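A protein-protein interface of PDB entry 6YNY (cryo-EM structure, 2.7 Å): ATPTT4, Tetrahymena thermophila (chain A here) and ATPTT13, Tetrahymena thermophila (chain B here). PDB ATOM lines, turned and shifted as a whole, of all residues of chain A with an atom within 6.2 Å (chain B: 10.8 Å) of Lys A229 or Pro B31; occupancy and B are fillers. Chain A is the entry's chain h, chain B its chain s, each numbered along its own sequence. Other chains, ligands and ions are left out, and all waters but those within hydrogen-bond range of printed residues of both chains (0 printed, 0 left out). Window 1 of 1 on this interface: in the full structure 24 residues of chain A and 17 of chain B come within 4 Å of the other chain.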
ATOM      1  N   TYR A 196      -4.338  23.241   8.913  1.00  0.00           N
ATOM      2  CA  TYR A 196      -5.450  23.235   9.853  1.00  0.00           C
ATOM      3  C   TYR A 196      -6.388  24.408   9.615  1.00  0.00           C
ATOM      4  O   TYR A 196      -7.582  24.317   9.914  1.00  0.00           O
ATOM      5  CB  TYR A 196      -4.922  23.258  11.283  1.00  0.00           C
ATOM      6  CG  TYR A 196      -5.987  23.075  12.334  1.00  0.00           C
ATOM      7  CD1 TYR A 196      -6.601  21.849  12.519  1.00  0.00           C
ATOM      8  CD2 TYR A 196      -6.370  24.125  13.150  1.00  0.00           C
ATOM      9  CE1 TYR A 196      -7.571  21.676  13.477  1.00  0.00           C
ATOM     10  CE2 TYR A 196      -7.338  23.960  14.113  1.00  0.00           C
ATOM     11  CZ  TYR A 196      -7.936  22.734  14.273  1.00  0.00           C
ATOM     12  OH  TYR A 196      -8.903  22.564  15.233  1.00  0.00           O
ATOM     13  N   LEU A 224      -6.915  33.817  14.542  1.00  0.00           N
ATOM     14  CA  LEU A 224      -6.506  34.285  15.860  1.00  0.00           C
ATOM     15  C   LEU A 224      -6.928  33.312  16.948  1.00  0.00           C
ATOM     16  O   LEU A 224      -6.164  33.044  17.882  1.00  0.00           O
ATOM     17  CB  LEU A 224      -7.091  35.667  16.132  1.00  0.00           C
ATOM     18  CG  LEU A 224      -6.723  36.760  15.136  1.00  0.00           C
ATOM     19  CD1 LEU A 224      -7.220  38.089  15.644  1.00  0.00           C
ATOM     20  CD2 LEU A 224      -5.233  36.800  14.895  1.00  0.00           C
ATOM     21  N   HIS A 225      -8.141  32.771  16.848  1.00  0.00           N
ATOM     22  CA  HIS A 225      -8.583  31.788  17.826  1.00  0.00           C
ATOM     23  C   HIS A 225      -7.638  30.596  17.863  1.00  0.00           C
ATOM     24  O   HIS A 225      -7.340  30.061  18.936  1.00  0.00           O
ATOM     25  CB  HIS A 225     -10.000  31.333  17.504  1.00  0.00           C
ATOM     26  CG  HIS A 225     -10.560  30.368  18.496  1.00  0.00           C
ATOM     27  ND1 HIS A 225     -11.079  30.765  19.708  1.00  0.00           N
ATOM     28  CD2 HIS A 225     -10.674  29.020  18.460  1.00  0.00           C
ATOM     29  CE1 HIS A 225     -11.494  29.703  20.374  1.00  0.00           C
ATOM     30  NE2 HIS A 225     -11.259  28.632  19.639  1.00  0.00           N
ATOM     31  N   VAL A 226      -7.152  30.172  16.698  1.00  0.00           N
ATOM     32  CA  VAL A 226      -6.184  29.086  16.652  1.00  0.00           C
ATOM     33  C   VAL A 226      -4.849  29.540  17.222  1.00  0.00           C
ATOM     34  O   VAL A 226      -4.171  28.788  17.931  1.00  0.00           O
ATOM     35  CB  VAL A 226      -6.038  28.574  15.210  1.00  0.00           C
ATOM     36  CG1 VAL A 226      -4.928  27.555  15.117  1.00  0.00           C
ATOM     37  CG2 VAL A 226      -7.342  27.983  14.729  1.00  0.00           C
ATOM     38  N   PHE A 227      -4.450  30.777  16.921  1.00  0.00           N
ATOM     39  CA  PHE A 227      -3.187  31.289  17.434  1.00  0.00           C
ATOM     40  C   PHE A 227      -3.181  31.337  18.955  1.00  0.00           C
ATOM     41  O   PHE A 227      -2.199  30.939  19.591  1.00  0.00           O
ATOM     42  CB  PHE A 227      -2.913  32.677  16.862  1.00  0.00           C
ATOM     43  CG  PHE A 227      -2.624  32.692  15.389  1.00  0.00           C
ATOM     44  CD1 PHE A 227      -2.364  33.884  14.745  1.00  0.00           C
ATOM     45  CD2 PHE A 227      -2.620  31.528  14.647  1.00  0.00           C
ATOM     46  CE1 PHE A 227      -2.098  33.912  13.399  1.00  0.00           C
ATOM     47  CE2 PHE A 227      -2.356  31.556  13.301  1.00  0.00           C
ATOM     48  CZ  PHE A 227      -2.096  32.749  12.677  1.00  0.00           C
ATOM     49  N   ARG A 228      -4.264  31.828  19.559  1.00  0.00           N
ATOM     50  CA  ARG A 228      -4.314  31.917  21.013  1.00  0.00           C
ATOM     51  C   ARG A 228      -4.192  30.543  21.652  1.00  0.00           C
ATOM     52  O   ARG A 228      -3.553  30.391  22.699  1.00  0.00           O
ATOM     53  CB  ARG A 228      -5.603  32.606  21.454  1.00  0.00           C
ATOM     54  CG  ARG A 228      -5.725  34.017  20.944  1.00  0.00           C
ATOM     55  CD  ARG A 228      -6.861  34.773  21.589  1.00  0.00           C
ATOM     56  NE  ARG A 228      -7.089  36.048  20.916  1.00  0.00           N
ATOM     57  CZ  ARG A 228      -8.014  36.261  19.989  1.00  0.00           C
ATOM     58  NH1 ARG A 228      -8.831  35.291  19.612  1.00  0.00           N
ATOM     59  NH2 ARG A 228      -8.127  37.457  19.436  1.00  0.00           N
ATOM     60  N   LYS A 229      -4.798  29.530  21.039  1.00  0.00           N
ATOM     61  CA  LYS A 229      -4.683  28.178  21.569  1.00  0.00           C
ATOM     62  C   LYS A 229      -3.298  27.607  21.300  1.00  0.00           C
ATOM     63  O   LYS A 229      -2.751  26.870  22.127  1.00  0.00           O
ATOM     64  CB  LYS A 229      -5.776  27.296  20.971  1.00  0.00           C
ATOM     65  CG  LYS A 229      -6.191  26.130  21.847  1.00  0.00           C
ATOM     66  CD  LYS A 229      -7.677  25.832  21.710  1.00  0.00           C
ATOM     67  CE  LYS A 229      -8.043  25.317  20.332  1.00  0.00           C
ATOM     68  NZ  LYS A 229      -7.464  23.976  20.056  1.00  0.00           N
ATOM     69  N   ALA A 230      -2.713  27.942  20.151  1.00  0.00           N
ATOM     70  CA  ALA A 230      -1.355  27.504  19.855  1.00  0.00           C
ATOM     71  C   ALA A 230      -0.337  28.267  20.690  1.00  0.00           C
ATOM     72  O   ALA A 230       0.674  27.700  21.117  1.00  0.00           O
ATOM     73  CB  ALA A 230      -1.064  27.680  18.370  1.00  0.00           C
ATOM     74  N   ARG A 231      -0.581  29.556  20.921  1.00  0.00           N
ATOM     75  CA  ARG A 231       0.325  30.345  21.746  1.00  0.00           C
ATOM     76  C   ARG A 231       0.397  29.787  23.159  1.00  0.00           C
ATOM     77  O   ARG A 231       1.483  29.649  23.732  1.00  0.00           O
ATOM     78  CB  ARG A 231      -0.127  31.804  21.759  1.00  0.00           C
ATOM     79  CG  ARG A 231       0.531  32.644  22.824  1.00  0.00           C
ATOM     80  CD  ARG A 231       0.276  34.118  22.612  1.00  0.00           C
ATOM     81  NE  ARG A 231       1.026  34.638  21.476  1.00  0.00           N
ATOM     82  CZ  ARG A 231       2.311  34.979  21.522  1.00  0.00           C
ATOM     83  NH1 ARG A 231       2.998  34.858  22.651  1.00  0.00           N
ATOM     84  NH2 ARG A 231       2.913  35.443  20.437  1.00  0.00           N
ATOM     85  N   ALA A 232      -0.756  29.466  23.743  1.00  0.00           N
ATOM     86  CA  ALA A 232      -0.772  28.868  25.068  1.00  0.00           C
ATOM     87  C   ALA A 232      -0.240  27.444  25.056  1.00  0.00           C
ATOM     88  O   ALA A 232       0.147  26.929  26.109  1.00  0.00           O
ATOM     89  CB  ALA A 232      -2.190  28.888  25.629  1.00  0.00           C
ATOM     90  N   GLY A 233      -0.218  26.800  23.890  1.00  0.00           N
ATOM     91  CA  GLY A 233       0.288  25.444  23.806  1.00  0.00           C
ATOM     92  C   GLY A 233       1.790  25.354  23.956  1.00  0.00           C
ATOM     93  O   GLY A 233       2.310  24.331  24.407  1.00  0.00           O
ATOM     94  N   LYS A 234       2.508  26.404  23.570  1.00  0.00           N
ATOM     95  CA  LYS A 234       3.961  26.379  23.668  1.00  0.00           C
ATOM     96  C   LYS A 234       4.407  26.196  25.110  1.00  0.00           C
ATOM     97  O   LYS A 234       5.264  25.356  25.408  1.00  0.00           O
ATOM     98  CB  LYS A 234       4.536  27.664  23.083  1.00  0.00           C
ATOM     99  CG  LYS A 234       4.232  27.852  21.617  1.00  0.00           C
ATOM    100  CD  LYS A 234       4.839  29.133  21.093  1.00  0.00           C
ATOM    101  CE  LYS A 234       4.550  29.329  19.619  1.00  0.00           C
ATOM    102  NZ  LYS A 234       5.174  30.575  19.110  1.00  0.00           N
ATOM    103  N   ARG A 242      -7.179  16.271  24.583  1.00  0.00           N
ATOM    104  CA  ARG A 242      -7.622  17.549  25.124  1.00  0.00           C
ATOM    105  C   ARG A 242      -7.075  18.716  24.316  1.00  0.00           C
ATOM    106  O   ARG A 242      -7.770  19.715  24.100  1.00  0.00           O
ATOM    107  CB  ARG A 242      -7.196  17.661  26.585  1.00  0.00           C
ATOM    108  CG  ARG A 242      -7.919  16.698  27.494  1.00  0.00           C
ATOM    109  CD  ARG A 242      -7.342  16.700  28.888  1.00  0.00           C
ATOM    110  NE  ARG A 242      -6.096  15.951  28.970  1.00  0.00           N
ATOM    111  CZ  ARG A 242      -5.453  15.696  30.102  1.00  0.00           C
ATOM    112  NH1 ARG A 242      -5.938  16.129  31.254  1.00  0.00           N
ATOM    113  NH2 ARG A 242      -4.327  15.003  30.085  1.00  0.00           N
ATOM    114  N   GLY A 243      -5.829  18.609  23.865  1.00  0.00           N
ATOM    115  CA  GLY A 243      -5.234  19.619  23.029  1.00  0.00           C
ATOM    116  C   GLY A 243      -4.239  20.469  23.784  1.00  0.00           C
ATOM    117  O   GLY A 243      -3.887  20.187  24.933  1.00  0.00           O
ATOM    118  N   PRO A 244      -3.754  21.530  23.143  1.00  0.00           N
ATOM    119  CA  PRO A 244      -2.800  22.420  23.814  1.00  0.00           C
ATOM    120  C   PRO A 244      -3.453  23.134  24.987  1.00  0.00           C
ATOM    121  O   PRO A 244      -4.528  23.720  24.854  1.00  0.00           O
ATOM    122  CB  PRO A 244      -2.391  23.402  22.711  1.00  0.00           C
ATOM    123  CG  PRO A 244      -2.787  22.752  21.436  1.00  0.00           C
ATOM    124  CD  PRO A 244      -3.985  21.931  21.747  1.00  0.00           C
ATOM    125  N   ASP A 245      -2.790  23.085  26.140  1.00  0.00           N
ATOM    126  CA  ASP A 245      -3.265  23.766  27.340  1.00  0.00           C
ATOM    127  C   ASP A 245      -4.707  23.373  27.652  1.00  0.00           C
ATOM    128  O   ASP A 245      -5.586  24.218  27.831  1.00  0.00           O
ATOM    129  CB  ASP A 245      -3.130  25.279  27.186  1.00  0.00           C
ATOM    130  CG  ASP A 245      -3.367  26.018  28.482  1.00  0.00           C
ATOM    131  OD1 ASP A 245      -3.665  25.366  29.503  1.00  0.00           O
ATOM    132  OD2 ASP A 245      -3.245  27.257  28.482  1.00  0.00           O
ATOM    133  N   LEU B  22      -1.442  16.246  14.098  1.00  0.00           N
ATOM    134  CA  LEU B  22      -1.211  16.390  15.531  1.00  0.00           C
ATOM    135  C   LEU B  22      -2.482  16.820  16.254  1.00  0.00           C
ATOM    136  O   LEU B  22      -3.491  17.133  15.625  1.00  0.00           O
ATOM    137  CB  LEU B  22      -0.096  17.401  15.794  1.00  0.00           C
ATOM    138  CG  LEU B  22      -0.361  18.850  15.386  1.00  0.00           C
ATOM    139  CD1 LEU B  22       0.697  19.759  15.971  1.00  0.00           C
ATOM    140  CD2 LEU B  22      -0.396  18.990  13.879  1.00  0.00           C
ATOM    141  N   GLN B  23      -2.421  16.835  17.581  1.00  0.00           N
ATOM    142  CA  GLN B  23      -3.579  17.187  18.389  1.00  0.00           C
ATOM    143  C   GLN B  23      -3.835  18.687  18.358  1.00  0.00           C
ATOM    144  O   GLN B  23      -2.910  19.494  18.483  1.00  0.00           O
ATOM    145  CB  GLN B  23      -3.376  16.729  19.831  1.00  0.00           C
ATOM    146  CG  GLN B  23      -3.247  15.228  20.000  1.00  0.00           C
ATOM    147  CD  GLN B  23      -4.557  14.502  19.792  1.00  0.00           C
ATOM    148  OE1 GLN B  23      -5.531  15.077  19.308  1.00  0.00           O
ATOM    149  NE2 GLN B  23      -4.591  13.230  20.167  1.00  0.00           N
ATOM    150  N   TRP B  24      -5.106  19.053  18.193  1.00  0.00           N
ATOM    151  CA  TRP B  24      -5.528  20.445  18.194  1.00  0.00           C
ATOM    152  C   TRP B  24      -6.616  20.751  19.209  1.00  0.00           C
ATOM    153  O   TRP B  24      -6.868  21.931  19.478  1.00  0.00           O
ATOM    154  CB  TRP B  24      -6.023  20.858  16.802  1.00  0.00           C
ATOM    155  CG  TRP B  24      -4.943  20.908  15.784  1.00  0.00           C
ATOM    156  CD1 TRP B  24      -4.667  19.975  14.834  1.00  0.00           C
ATOM    157  CD2 TRP B  24      -3.983  21.951  15.616  1.00  0.00           C
ATOM    158  NE1 TRP B  24      -3.593  20.372  14.079  1.00  0.00           N
ATOM    159  CE2 TRP B  24      -3.154  21.585  14.541  1.00  0.00           C
ATOM    160  CE3 TRP B  24      -3.744  23.161  16.269  1.00  0.00           C
ATOM    161  CZ2 TRP B  24      -2.105  22.384  14.106  1.00  0.00           C
ATOM    162  CZ3 TRP B  24      -2.704  23.952  15.837  1.00  0.00           C
ATOM    163  CH2 TRP B  24      -1.895  23.562  14.765  1.00  0.00           C
ATOM    164  N   GLY B  25      -7.261  19.742  19.776  1.00  0.00           N
ATOM    165  CA  GLY B  25      -8.317  19.981  20.732  1.00  0.00           C
ATOM    166  C   GLY B  25      -9.604  20.406  20.047  1.00  0.00           C
ATOM    167  O   GLY B  25      -9.849  20.118  18.871  1.00  0.00           O
ATOM    168  N   SER B  26     -10.436  21.106  20.808  1.00  0.00           N
ATOM    169  CA  SER B  26     -11.720  21.591  20.321  1.00  0.00           C
ATOM    170  C   SER B  26     -11.567  23.024  19.835  1.00  0.00           C
ATOM    171  O   SER B  26     -11.094  23.890  20.578  1.00  0.00           O
ATOM    172  CB  SER B  26     -12.781  21.512  21.418  1.00  0.00           C
ATOM    173  OG  SER B  26     -14.041  21.946  20.941  1.00  0.00           O
ATOM    174  N   LEU B  27     -11.967  23.267  18.587  1.00  0.00           N
ATOM    175  CA  LEU B  27     -11.916  24.620  18.048  1.00  0.00           C
ATOM    176  C   LEU B  27     -12.736  25.580  18.896  1.00  0.00           C
ATOM    177  O   LEU B  27     -12.332  26.727  19.116  1.00  0.00           O
ATOM    178  CB  LEU B  27     -12.421  24.625  16.608  1.00  0.00           C
ATOM    179  CG  LEU B  27     -12.456  25.981  15.904  1.00  0.00           C
ATOM    180  CD1 LEU B  27     -11.080  26.345  15.396  1.00  0.00           C
ATOM    181  CD2 LEU B  27     -13.478  25.980  14.783  1.00  0.00           C
ATOM    182  N   ALA B  28     -13.896  25.134  19.374  1.00  0.00           N
ATOM    183  CA  ALA B  28     -14.764  26.019  20.141  1.00  0.00           C
ATOM    184  C   ALA B  28     -14.113  26.428  21.455  1.00  0.00           C
ATOM    185  O   ALA B  28     -14.082  27.613  21.801  1.00  0.00           O
ATOM    186  CB  ALA B  28     -16.103  25.337  20.398  1.00  0.00           C
ATOM    187  N   GLU B  29     -13.584  25.461  22.198  1.00  0.00           N
ATOM    188  CA  GLU B  29     -13.008  25.754  23.500  1.00  0.00           C
ATOM    189  C   GLU B  29     -11.824  26.704  23.369  1.00  0.00           C
ATOM    190  O   GLU B  29     -11.075  26.672  22.390  1.00  0.00           O
ATOM    191  CB  GLU B  29     -12.564  24.464  24.187  1.00  0.00           C
ATOM    192  CG  GLU B  29     -13.682  23.478  24.442  1.00  0.00           C
ATOM    193  CD  GLU B  29     -13.192  22.197  25.081  1.00  0.00           C
ATOM    194  OE1 GLU B  29     -11.961  22.035  25.222  1.00  0.00           O
ATOM    195  OE2 GLU B  29     -14.036  21.351  25.442  1.00  0.00           O
ATOM    196  N   ARG B  30     -11.669  27.561  24.371  1.00  0.00           N
ATOM    197  CA  ARG B  30     -10.517  28.448  24.455  1.00  0.00           C
ATOM    198  C   ARG B  30      -9.449  27.786  25.314  1.00  0.00           C
ATOM    199  O   ARG B  30      -9.685  26.708  25.872  1.00  0.00           O
ATOM    200  CB  ARG B  30     -10.910  29.793  25.056  1.00  0.00           C
ATOM    201  CG  ARG B  30     -12.154  30.398  24.485  1.00  0.00           C
ATOM    202  CD  ARG B  30     -12.321  31.804  25.001  1.00  0.00           C
ATOM    203  NE  ARG B  30     -11.338  32.713  24.426  1.00  0.00           N
ATOM    204  CZ  ARG B  30     -11.024  33.895  24.940  1.00  0.00           C
ATOM    205  NH1 ARG B  30     -11.606  34.316  26.049  1.00  0.00           N
ATOM    206  NH2 ARG B  30     -10.122  34.656  24.345  1.00  0.00           N
ATOM    207  N   PRO B  31      -8.269  28.387  25.448  1.00  0.00           N
ATOM    208  CA  PRO B  31      -7.273  27.835  26.366  1.00  0.00           C
ATOM    209  C   PRO B  31      -7.811  27.756  27.784  1.00  0.00           C
ATOM    210  O   PRO B  31      -8.626  28.575  28.210  1.00  0.00           O
ATOM    211  CB  PRO B  31      -6.110  28.823  26.263  1.00  0.00           C
ATOM    212  CG  PRO B  31      -6.268  29.454  24.955  1.00  0.00           C
ATOM    213  CD  PRO B  31      -7.731  29.528  24.692  1.00  0.00           C
ATOM    214  N   MET B  32      -7.341  26.749  28.519  1.00  0.00           N
ATOM    215  CA  MET B  32      -7.814  26.549  29.881  1.00  0.00           C
ATOM    216  C   MET B  32      -7.476  27.725  30.784  1.00  0.00           C
ATOM    217  O   MET B  32      -8.110  27.890  31.831  1.00  0.00           O
ATOM    218  CB  MET B  32      -7.226  25.259  30.445  1.00  0.00           C
ATOM    219  CG  MET B  32      -7.751  24.883  31.815  1.00  0.00           C
ATOM    220  SD  MET B  32      -9.542  24.716  31.862  1.00  0.00           S
ATOM    221  CE  MET B  32      -9.746  23.264  30.845  1.00  0.00           C
ATOM    222  N   VAL B  33      -6.496  28.547  30.404  1.00  0.00           N
ATOM    223  CA  VAL B  33      -6.134  29.702  31.222  1.00  0.00           C
ATOM    224  C   VAL B  33      -7.308  30.661  31.325  1.00  0.00           C
ATOM    225  O   VAL B  33      -7.604  31.195  32.401  1.00  0.00           O
ATOM    226  CB  VAL B  33      -4.896  30.416  30.647  1.00  0.00           C
ATOM    227  CG1 VAL B  33      -4.209  31.223  31.726  1.00  0.00           C
ATOM    228  CG2 VAL B  33      -3.941  29.441  30.032  1.00  0.00           C
ATOM    229  N   ASP B  34      -7.991  30.902  30.206  1.00  0.00           N
ATOM    230  CA  ASP B  34      -9.114  31.829  30.205  1.00  0.00           C
ATOM    231  C   ASP B  34     -10.286  31.294  31.015  1.00  0.00           C
ATOM    232  O   ASP B  34     -11.102  32.076  31.511  1.00  0.00           O
ATOM    233  CB  ASP B  34      -9.545  32.109  28.768  1.00  0.00           C
ATOM    234  CG  ASP B  34      -8.421  32.667  27.921  1.00  0.00           C
ATOM    235  OD1 ASP B  34      -7.305  32.838  28.451  1.00  0.00           O
ATOM    236  OD2 ASP B  34      -8.652  32.934  26.724  1.00  0.00           O
ATOM    237  N   ARG B  35     -10.386  29.976  31.154  1.00  0.00           N
ATOM    238  CA  ARG B  35     -11.487  29.356  31.875  1.00  0.00           C
ATOM    239  C   ARG B  35     -11.197  29.193  33.357  1.00  0.00           C
ATOM    240  O   ARG B  35     -12.127  29.201  34.171  1.00  0.00           O
ATOM    241  CB  ARG B  35     -11.799  27.991  31.265  1.00  0.00           C
ATOM    242  CG  ARG B  35     -12.260  28.055  29.828  1.00  0.00           C
ATOM    243  CD  ARG B  35     -12.473  26.677  29.252  1.00  0.00           C
ATOM    244  NE  ARG B  35     -11.305  26.172  28.543  1.00  0.00           N
ATOM    245  CZ  ARG B  35     -11.149  24.906  28.174  1.00  0.00           C
ATOM    246  NH1 ARG B  35     -12.083  24.011  28.460  1.00  0.00           N
ATOM    247  NH2 ARG B  35     -10.059  24.531  27.523  1.00  0.00           N
ATOM    248  N   VAL B  36      -9.933  29.038  33.715  1.00  0.00           N
ATOM    249  CA  VAL B  36      -9.537  28.766  35.091  1.00  0.00           C
ATOM    250  C   VAL B  36      -9.542  30.063  35.888  1.00  0.00           C
ATOM    251  O   VAL B  36      -8.900  31.044  35.501  1.00  0.00           O
ATOM    252  CB  VAL B  36      -8.159  28.092  35.114  1.00  0.00           C
ATOM    253  CG1 VAL B  36      -7.435  28.405  36.367  1.00  0.00           C
ATOM    254  CG2 VAL B  36      -8.318  26.600  34.962  1.00  0.00           C
ATOM    255  N   MET B  37     -10.252  30.065  37.015  1.00  0.00           N
ATOM    256  CA  MET B  37     -10.477  31.272  37.796  1.00  0.00           C
ATOM    257  C   MET B  37     -10.128  31.029  39.259  1.00  0.00           C
ATOM    258  O   MET B  37      -9.924  29.895  39.699  1.00  0.00           O
ATOM    259  CB  MET B  37     -11.934  31.743  37.697  1.00  0.00           C
ATOM    260  CG  MET B  37     -12.612  31.460  36.370  1.00  0.00           C
ATOM    261  SD  MET B  37     -11.805  32.204  34.947  1.00  0.00           S
ATOM    262  CE  MET B  37     -12.199  33.912  35.230  1.00  0.00           C
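Among the printed residues, merely in contact across the chains: Asp A245 with Val B33 (2.8 Å), Lys A229 with Ser B26 (3.4 Å), Arg A242 with Gly B25 (3.4 Å), Tyr A196 with Trp B24 (3.6 Å), Lys A229 with Glu B29 (3.6 Å), His A225 with Ala B28 (3.6 Å), Arg A228 with Pro B31 (3.7 Å), Pro A244 with Trp B24 (3.7 Å), Gly A243 with Gly B25 (3.8 Å), Asp A245 with Pro B31 (3.9 Å), Lys A229 with Pro B31 (3.95 Å) and Ala A232 with Pro B31 (3.97 Å).
The side-chain carboxylate (OE1) of Glu B29 is in salt-bridge range of the guanidinium group (NH1) of Arg B35, 3.8 Å away.
Of the 16 printed residues of chain B, 9 touch a printed residue of chain A. Of the 16 printed residues of chain A, 9 touch a printed residue of chain B. Hydrophobic or aromatic side chains of chain A within 4 Å of the printed part of chain B: Tyr A196, His A225, Ala A232 and Pro A244. Among the printed residues, 16 pairs touch across the chains.
Lys A229 touches just these residues of chain B: Trp B24, Ser B26, Glu B29 and Pro B31. No residue of chain B comes within 4 Å of Val A226. Of the printed residues of chain B, Ala A232 touches Pro B31. Of chain B, only Trp B24 comes within 4 Å of Pro A244. Printed residues of chain B within 4 Å of Tyr A196: Trp B24. Printed residues of chain A within 4 Å of Ser B26: Lys A229. Of the printed residues of chain A, Leu B27 touches His A225. Of the printed residues of chain A, Glu B29 touches His A225 (3.4 Å) and Lys A229 (3.6 Å). Of the printed residues of chain A, Met B32 touches Asp A245 (3.2 Å). The nearest residue of chain A that does not touch Pro B31 is Pro A244 (5.2 Å).
NZ of Lys A229 sits close to O of Trp B24, 2.2 Å away. NE2 of His A225 sits at hydrogen-bond distance from O of Glu B29. O of Leu B27 lies close to NE2 of His A225, at 2.2 Å. The backbone NH of Met B32 is in hydrogen-bond range of the backbone carbonyl oxygen of Asp A245.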
